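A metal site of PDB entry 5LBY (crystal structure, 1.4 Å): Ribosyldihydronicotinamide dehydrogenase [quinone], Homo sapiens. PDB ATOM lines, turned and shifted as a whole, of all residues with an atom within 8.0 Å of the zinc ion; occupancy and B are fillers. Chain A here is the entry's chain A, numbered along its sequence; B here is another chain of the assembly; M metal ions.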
ATOM      1  N   TYR A 133     -36.408  10.536  -8.463  1.00  0.00           N
ATOM      2  CA  TYR A 133     -35.354  10.732  -9.487  1.00  0.00           C
ATOM      3  C   TYR A 133     -35.971  10.823 -10.846  1.00  0.00           C
ATOM      4  O   TYR A 133     -36.901  11.589 -11.007  1.00  0.00           O
ATOM      5  CB  TYR A 133     -34.158   9.790  -9.324  1.00  0.00           C
ATOM      6  CG  TYR A 133     -33.376  10.104  -8.053  1.00  0.00           C
ATOM      7  CD1 TYR A 133     -32.762  11.337  -7.890  1.00  0.00           C
ATOM      8  CD2 TYR A 133     -33.259   9.202  -7.043  1.00  0.00           C
ATOM      9  CE1 TYR A 133     -32.085  11.674  -6.738  1.00  0.00           C
ATOM     10  CE2 TYR A 133     -32.552   9.499  -5.859  1.00  0.00           C
ATOM     11  CZ  TYR A 133     -31.975  10.764  -5.728  1.00  0.00           C
ATOM     12  OH  TYR A 133     -31.290  11.135  -4.591  1.00  0.00           O
ATOM     13  N   ASP A 134     -35.521  10.046 -11.804  1.00  0.00           N
ATOM     14  CA  ASP A 134     -36.077  10.232 -13.147  1.00  0.00           C
ATOM     15  C   ASP A 134     -37.547   9.924 -13.230  1.00  0.00           C
ATOM     16  O   ASP A 134     -38.201  10.404 -14.182  1.00  0.00           O
ATOM     17  CB  ASP A 134     -35.302   9.428 -14.171  1.00  0.00           C
ATOM     18  CG  ASP A 134     -33.944   9.939 -14.507  1.00  0.00           C
ATOM     19  OD1 ASP A 134     -33.471  10.932 -13.960  1.00  0.00           O
ATOM     20  OD2 ASP A 134     -33.327   9.246 -15.348  1.00  0.00           O
ATOM     21  N   TRP A 170     -25.009  19.870  -4.700  1.00  0.00           N
ATOM     22  CA  TRP A 170     -25.580  18.500  -4.664  1.00  0.00           C
ATOM     23  C   TRP A 170     -26.944  18.357  -3.962  1.00  0.00           C
ATOM     24  O   TRP A 170     -27.840  17.788  -4.532  1.00  0.00           O
ATOM     25  CB  TRP A 170     -24.530  17.579  -4.073  1.00  0.00           C
ATOM     26  CG  TRP A 170     -24.914  16.203  -3.733  1.00  0.00           C
ATOM     27  CD1 TRP A 170     -25.143  15.654  -2.508  1.00  0.00           C
ATOM     28  CD2 TRP A 170     -25.043  15.111  -4.674  1.00  0.00           C
ATOM     29  NE1 TRP A 170     -25.416  14.318  -2.621  1.00  0.00           N
ATOM     30  CE2 TRP A 170     -25.362  13.940  -3.943  1.00  0.00           C
ATOM     31  CE3 TRP A 170     -24.975  15.021  -6.082  1.00  0.00           C
ATOM     32  CZ2 TRP A 170     -25.551  12.724  -4.531  1.00  0.00           C
ATOM     33  CZ3 TRP A 170     -25.143  13.771  -6.655  1.00  0.00           C
ATOM     34  CH2 TRP A 170     -25.405  12.645  -5.888  1.00  0.00           C
ATOM     35  N   LEU A 172     -29.229  20.451  -3.477  1.00  0.00           N
ATOM     36  CA  LEU A 172     -30.223  21.223  -4.201  1.00  0.00           C
ATOM     37  C   LEU A 172     -30.529  20.608  -5.533  1.00  0.00           C
ATOM     38  O   LEU A 172     -31.663  20.249  -5.838  1.00  0.00           O
ATOM     39  CB  LEU A 172     -29.784  22.686  -4.336  1.00  0.00           C
ATOM     40  CG  LEU A 172     -29.512  23.444  -3.038  1.00  0.00           C
ATOM     41  CD1 LEU A 172     -28.895  24.803  -3.361  1.00  0.00           C
ATOM     42  CD2 LEU A 172     -30.757  23.611  -2.256  1.00  0.00           C
ATOM     43  N   GLN A 173     -29.507  20.485  -6.383  1.00  0.00           N
ATOM     44  CA  GLN A 173     -29.720  19.959  -7.735  1.00  0.00           C
ATOM     45  C   GLN A 173     -30.125  18.509  -7.731  1.00  0.00           C
ATOM     46  O   GLN A 173     -31.076  18.150  -8.440  1.00  0.00           O
ATOM     47  CB  GLN A 173     -28.496  20.199  -8.577  1.00  0.00           C
ATOM     48  CG  GLN A 173     -28.219  21.684  -8.843  1.00  0.00           C
ATOM     49  CD  GLN A 173     -27.138  22.011  -9.816  1.00  0.00           C
ATOM     50  OE1 GLN A 173     -27.197  23.054 -10.441  1.00  0.00           O
ATOM     51  NE2 GLN A 173     -26.147  21.161  -9.948  1.00  0.00           N
ATOM     52  N   HIS A 174     -29.394  17.685  -7.011  1.00  0.00           N
ATOM     53  CA  HIS A 174     -29.638  16.261  -6.995  1.00  0.00           C
ATOM     54  C   HIS A 174     -30.652  15.830  -5.978  1.00  0.00           C
ATOM     55  O   HIS A 174     -31.655  15.189  -6.295  1.00  0.00           O
ATOM     56  CB  HIS A 174     -28.351  15.484  -6.807  1.00  0.00           C
ATOM     57  CG  HIS A 174     -28.534  14.023  -6.858  1.00  0.00           C
ATOM     58  ND1 HIS A 174     -28.670  13.350  -8.062  1.00  0.00           N
ATOM     59  CD2 HIS A 174     -28.557  13.085  -5.883  1.00  0.00           C
ATOM     60  CE1 HIS A 174     -28.748  12.049  -7.806  1.00  0.00           C
ATOM     61  NE2 HIS A 174     -28.697  11.875  -6.499  1.00  0.00           N
ATOM     62  N   GLY A 175     -30.402  16.199  -4.732  1.00  0.00           N
ATOM     63  CA  GLY A 175     -31.232  15.749  -3.647  1.00  0.00           C
ATOM     64  C   GLY A 175     -32.627  16.295  -3.673  1.00  0.00           C
ATOM     65  O   GLY A 175     -33.524  15.674  -3.102  1.00  0.00           O
ATOM     66  N   THR A 176     -32.820  17.469  -4.296  1.00  0.00           N
ATOM     67  CA  THR A 176     -34.158  18.054  -4.343  1.00  0.00           C
ATOM     68  C   THR A 176     -34.717  18.057  -5.761  1.00  0.00           C
ATOM     69  O   THR A 176     -35.713  17.398  -6.019  1.00  0.00           O
ATOM     70  CB  THR A 176     -34.143  19.483  -3.748  1.00  0.00           C
ATOM     71  OG1 THR A 176     -33.495  19.466  -2.479  1.00  0.00           O
ATOM     72  CG2 THR A 176     -35.552  20.001  -3.566  1.00  0.00           C
ATOM     73  N   LEU A 177     -34.068  18.781  -6.662  1.00  0.00           N
ATOM     74  CA  LEU A 177     -34.654  18.969  -8.004  1.00  0.00           C
ATOM     75  C   LEU A 177     -34.707  17.659  -8.806  1.00  0.00           C
ATOM     76  O   LEU A 177     -35.774  17.249  -9.285  1.00  0.00           O
ATOM     77  CB  LEU A 177     -33.912  20.077  -8.738  1.00  0.00           C
ATOM     78  CG  LEU A 177     -33.927  21.430  -8.054  1.00  0.00           C
ATOM     79  CD1 LEU A 177     -33.062  22.458  -8.814  1.00  0.00           C
ATOM     80  CD2 LEU A 177     -35.292  21.924  -7.818  1.00  0.00           C
ATOM     81  N   HIS A 178     -33.574  16.992  -8.959  1.00  0.00           N
ATOM     82  CA  HIS A 178     -33.569  15.703  -9.665  1.00  0.00           C
ATOM     83  C   HIS A 178     -34.464  14.715  -8.937  1.00  0.00           C
ATOM     84  O   HIS A 178     -35.178  13.920  -9.599  1.00  0.00           O
ATOM     85  CB  HIS A 178     -32.118  15.205  -9.769  1.00  0.00           C
ATOM     86  CG  HIS A 178     -31.929  13.981 -10.581  1.00  0.00           C
ATOM     87  ND1 HIS A 178     -30.729  13.391 -10.705  1.00  0.00           N
ATOM     88  CD2 HIS A 178     -32.800  13.249 -11.309  1.00  0.00           C
ATOM     89  CE1 HIS A 178     -30.840  12.297 -11.430  1.00  0.00           C
ATOM     90  NE2 HIS A 178     -32.096  12.203 -11.822  1.00  0.00           N
ATOM     91  N   PHE A 179     -34.443  14.683  -7.632  1.00  0.00           N
ATOM     92  CA  PHE A 179     -35.299  13.742  -6.894  1.00  0.00           C
ATOM     93  C   PHE A 179     -36.764  13.880  -7.292  1.00  0.00           C
ATOM     94  O   PHE A 179     -37.476  12.864  -7.342  1.00  0.00           O
ATOM     95  CB  PHE A 179     -35.133  13.992  -5.362  1.00  0.00           C
ATOM     96  CG  PHE A 179     -35.730  12.935  -4.490  1.00  0.00           C
ATOM     97  CD1 PHE A 179     -34.966  11.843  -4.107  1.00  0.00           C
ATOM     98  CD2 PHE A 179     -37.054  13.013  -4.060  1.00  0.00           C
ATOM     99  CE1 PHE A 179     -35.497  10.872  -3.291  1.00  0.00           C
ATOM    100  CE2 PHE A 179     -37.582  12.039  -3.235  1.00  0.00           C
ATOM    101  CZ  PHE A 179     -36.815  10.969  -2.879  1.00  0.00           C
ATOM    102  N   PHE A 182     -37.139  16.790 -11.997  1.00  0.00           N
ATOM    103  CA  PHE A 182     -36.678  17.854 -12.870  1.00  0.00           C
ATOM    104  C   PHE A 182     -35.431  17.420 -13.643  1.00  0.00           C
ATOM    105  O   PHE A 182     -34.591  16.698 -13.123  1.00  0.00           O
ATOM    106  CB  PHE A 182     -36.270  19.082 -12.096  1.00  0.00           C
ATOM    107  CG  PHE A 182     -37.400  19.876 -11.528  1.00  0.00           C
ATOM    108  CD1 PHE A 182     -38.074  20.763 -12.329  1.00  0.00           C
ATOM    109  CD2 PHE A 182     -37.765  19.788 -10.192  1.00  0.00           C
ATOM    110  CE1 PHE A 182     -39.072  21.551 -11.813  1.00  0.00           C
ATOM    111  CE2 PHE A 182     -38.746  20.574  -9.672  1.00  0.00           C
ATOM    112  CZ  PHE A 182     -39.413  21.454 -10.478  1.00  0.00           C
ATOM    113  N   VAL A 184     -32.113  19.454 -14.812  1.00  0.00           N
ATOM    114  CA  VAL A 184     -31.456  20.607 -14.211  1.00  0.00           C
ATOM    115  C   VAL A 184     -30.580  21.278 -15.304  1.00  0.00           C
ATOM    116  O   VAL A 184     -29.710  20.640 -15.859  1.00  0.00           O
ATOM    117  CB  VAL A 184     -30.606  20.180 -13.008  1.00  0.00           C
ATOM    118  CG1 VAL A 184     -29.864  21.374 -12.438  1.00  0.00           C
ATOM    119  CG2 VAL A 184     -31.518  19.541 -11.947  1.00  0.00           C
ATOM    120  N   ILE A 221     -27.777  19.440 -17.544  1.00  0.00           N
ATOM    121  CA  ILE A 221     -26.592  18.757 -17.067  1.00  0.00           C
ATOM    122  C   ILE A 221     -26.887  17.292 -16.766  1.00  0.00           C
ATOM    123  O   ILE A 221     -28.031  16.929 -16.524  1.00  0.00           O
ATOM    124  CB  ILE A 221     -26.032  19.427 -15.794  1.00  0.00           C
ATOM    125  CG1 ILE A 221     -26.940  19.175 -14.566  1.00  0.00           C
ATOM    126  CG2 ILE A 221     -25.766  20.883 -16.032  1.00  0.00           C
ATOM    127  CD1 ILE A 221     -26.346  19.578 -13.263  1.00  0.00           C
ATOM    128  N   PRO A 222     -25.867  16.444 -16.697  1.00  0.00           N
ATOM    129  CA  PRO A 222     -26.028  15.089 -16.181  1.00  0.00           C
ATOM    130  C   PRO A 222     -25.976  15.197 -14.669  1.00  0.00           C
ATOM    131  O   PRO A 222     -24.888  15.494 -14.109  1.00  0.00           O
ATOM    132  CB  PRO A 222     -24.829  14.341 -16.740  1.00  0.00           C
ATOM    133  CG  PRO A 222     -23.807  15.381 -16.990  1.00  0.00           C
ATOM    134  CD  PRO A 222     -24.545  16.635 -17.302  1.00  0.00           C
ATOM    135  N   CYS A 223     -27.093  15.076 -14.010  1.00  0.00           N
ATOM    136  CA  CYS A 223     -27.157  15.388 -12.582  1.00  0.00           C
ATOM    137  C   CYS A 223     -26.754  14.133 -11.808  1.00  0.00           C
ATOM    138  O   CYS A 223     -27.564  13.403 -11.203  1.00  0.00           O
ATOM    139  CB  CYS A 223     -28.537  15.921 -12.217  1.00  0.00           C
ATOM    140  SG  CYS A 223     -28.647  16.399 -10.478  1.00  0.00           S
ATOM    141  N   THR A 224     -25.442  13.903 -11.823  1.00  0.00           N
ATOM    142  CA  THR A 224     -24.834  12.713 -11.242  1.00  0.00           C
ATOM    143  C   THR A 224     -23.843  13.090 -10.154  1.00  0.00           C
ATOM    144  O   THR A 224     -23.363  14.234 -10.100  1.00  0.00           O
ATOM    145  CB  THR A 224     -24.117  11.906 -12.300  1.00  0.00           C
ATOM    146  OG1 THR A 224     -23.071  12.747 -12.841  1.00  0.00           O
ATOM    147  CG2 THR A 224     -25.063  11.473 -13.377  1.00  0.00           C
ATOM    148  N   ALA A 225     -23.497  12.117  -9.331  1.00  0.00           N
ATOM    149  CA  ALA A 225     -22.411  12.320  -8.398  1.00  0.00           C
ATOM    150  C   ALA A 225     -21.113  12.663  -9.127  1.00  0.00           C
ATOM    151  O   ALA A 225     -20.352  13.507  -8.702  1.00  0.00           O
ATOM    152  CB  ALA A 225     -22.230  11.108  -7.504  1.00  0.00           C
ATOM    153  N   TRP A 227     -20.755  14.393 -11.930  1.00  0.00           N
ATOM    154  CA  TRP A 227     -20.757  15.775 -12.331  1.00  0.00           C
ATOM    155  C   TRP A 227     -20.405  16.684 -11.141  1.00  0.00           C
ATOM    156  O   TRP A 227     -19.666  17.672 -11.287  1.00  0.00           O
ATOM    157  CB  TRP A 227     -22.130  16.172 -12.909  1.00  0.00           C
ATOM    158  CG  TRP A 227     -22.188  17.570 -13.462  1.00  0.00           C
ATOM    159  CD1 TRP A 227     -21.958  17.931 -14.754  1.00  0.00           C
ATOM    160  CD2 TRP A 227     -22.524  18.748 -12.751  1.00  0.00           C
ATOM    161  NE1 TRP A 227     -22.127  19.275 -14.880  1.00  0.00           N
ATOM    162  CE2 TRP A 227     -22.455  19.812 -13.684  1.00  0.00           C
ATOM    163  CE3 TRP A 227     -22.842  19.034 -11.422  1.00  0.00           C
ATOM    164  CZ2 TRP A 227     -22.700  21.140 -13.319  1.00  0.00           C
ATOM    165  CZ3 TRP A 227     -23.075  20.350 -11.065  1.00  0.00           C
ATOM    166  CH2 TRP A 227     -23.011  21.378 -11.974  1.00  0.00           C
ATOM    167  N   HIS A 228     -20.971  16.359  -9.976  1.00  0.00           N
ATOM    168  CA  HIS A 228     -20.772  17.231  -8.838  1.00  0.00           C
ATOM    169  C   HIS A 228     -19.371  17.076  -8.210  1.00  0.00           C
ATOM    170  O   HIS A 228     -18.833  18.083  -7.751  1.00  0.00           O
ATOM    171  CB  HIS A 228     -21.848  16.976  -7.779  1.00  0.00           C
ATOM    172  CG  HIS A 228     -23.199  17.463  -8.184  1.00  0.00           C
ATOM    173  ND1 HIS A 228     -24.077  16.734  -8.974  1.00  0.00           N
ATOM    174  CD2 HIS A 228     -23.837  18.623  -7.907  1.00  0.00           C
ATOM    175  CE1 HIS A 228     -25.183  17.447  -9.151  1.00  0.00           C
ATOM    176  NE2 HIS A 228     -25.062  18.580  -8.517  1.00  0.00           N
ATOM    177  N   VAL B 161     -28.730   5.165  -4.763  1.00  0.00           N
ATOM    178  CA  VAL B 161     -29.481   6.232  -5.481  1.00  0.00           C
ATOM    179  C   VAL B 161     -29.262   7.587  -4.897  1.00  0.00           C
ATOM    180  O   VAL B 161     -29.295   8.583  -5.623  1.00  0.00           O
ATOM    181  CB  VAL B 161     -30.991   5.907  -5.554  1.00  0.00           C
ATOM    182  CG1 VAL B 161     -31.286   4.793  -6.516  1.00  0.00           C
ATOM    183  CG2 VAL B 161     -31.614   5.671  -4.141  1.00  0.00           C
HETATM  184 ZN    ZN M   1     -28.993  14.219  -9.947  1.00  0.00          ZN
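Three residues have an atom within 4 Å of the zinc ion: His 174, His 178 and Cys 223.
The nearest printed residue that does not touch the zinc ion is Thr 224 (4.03 Å).
A ring nitrogen (ND1) of His 178 is bound to the zinc ion, 2.1 Å away.
The zinc ion is bound by O of Cys 223 (2.1 Å).
The zinc ion is bound by ND1 of His 174, at 2.1 Å.
SG of Cys 223 is bound to the zinc ion, at 2.3 Å.
The zinc ion has four donor atoms within binding distance.
The backbone NH of His 178 lies within hydrogen-bond range of the backbone carbonyl oxygen of Gln 173 (2.8 Å).
The side-chain carboxylate (OD1) of Asp 134 lies within hydrogen-bond range of a ring nitrogen (NE2) of His 178.
The side-chain sulfur of Cys 223 lies close to the backbone carbonyl oxygen of Gln 173 (3.6 Å).
NE2 of His 174 sits at hydrogen-bond distance from OH of Tyr 133 (3.3 Å).
The backbone carbonyl oxygen of His 174 is in hydrogen-bond range of the backbone NH of Phe 179 (3.1 Å).
O of Val 161 of chain B is in hydrogen-bond range of NE2 of His 174, at 3.5 Å.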
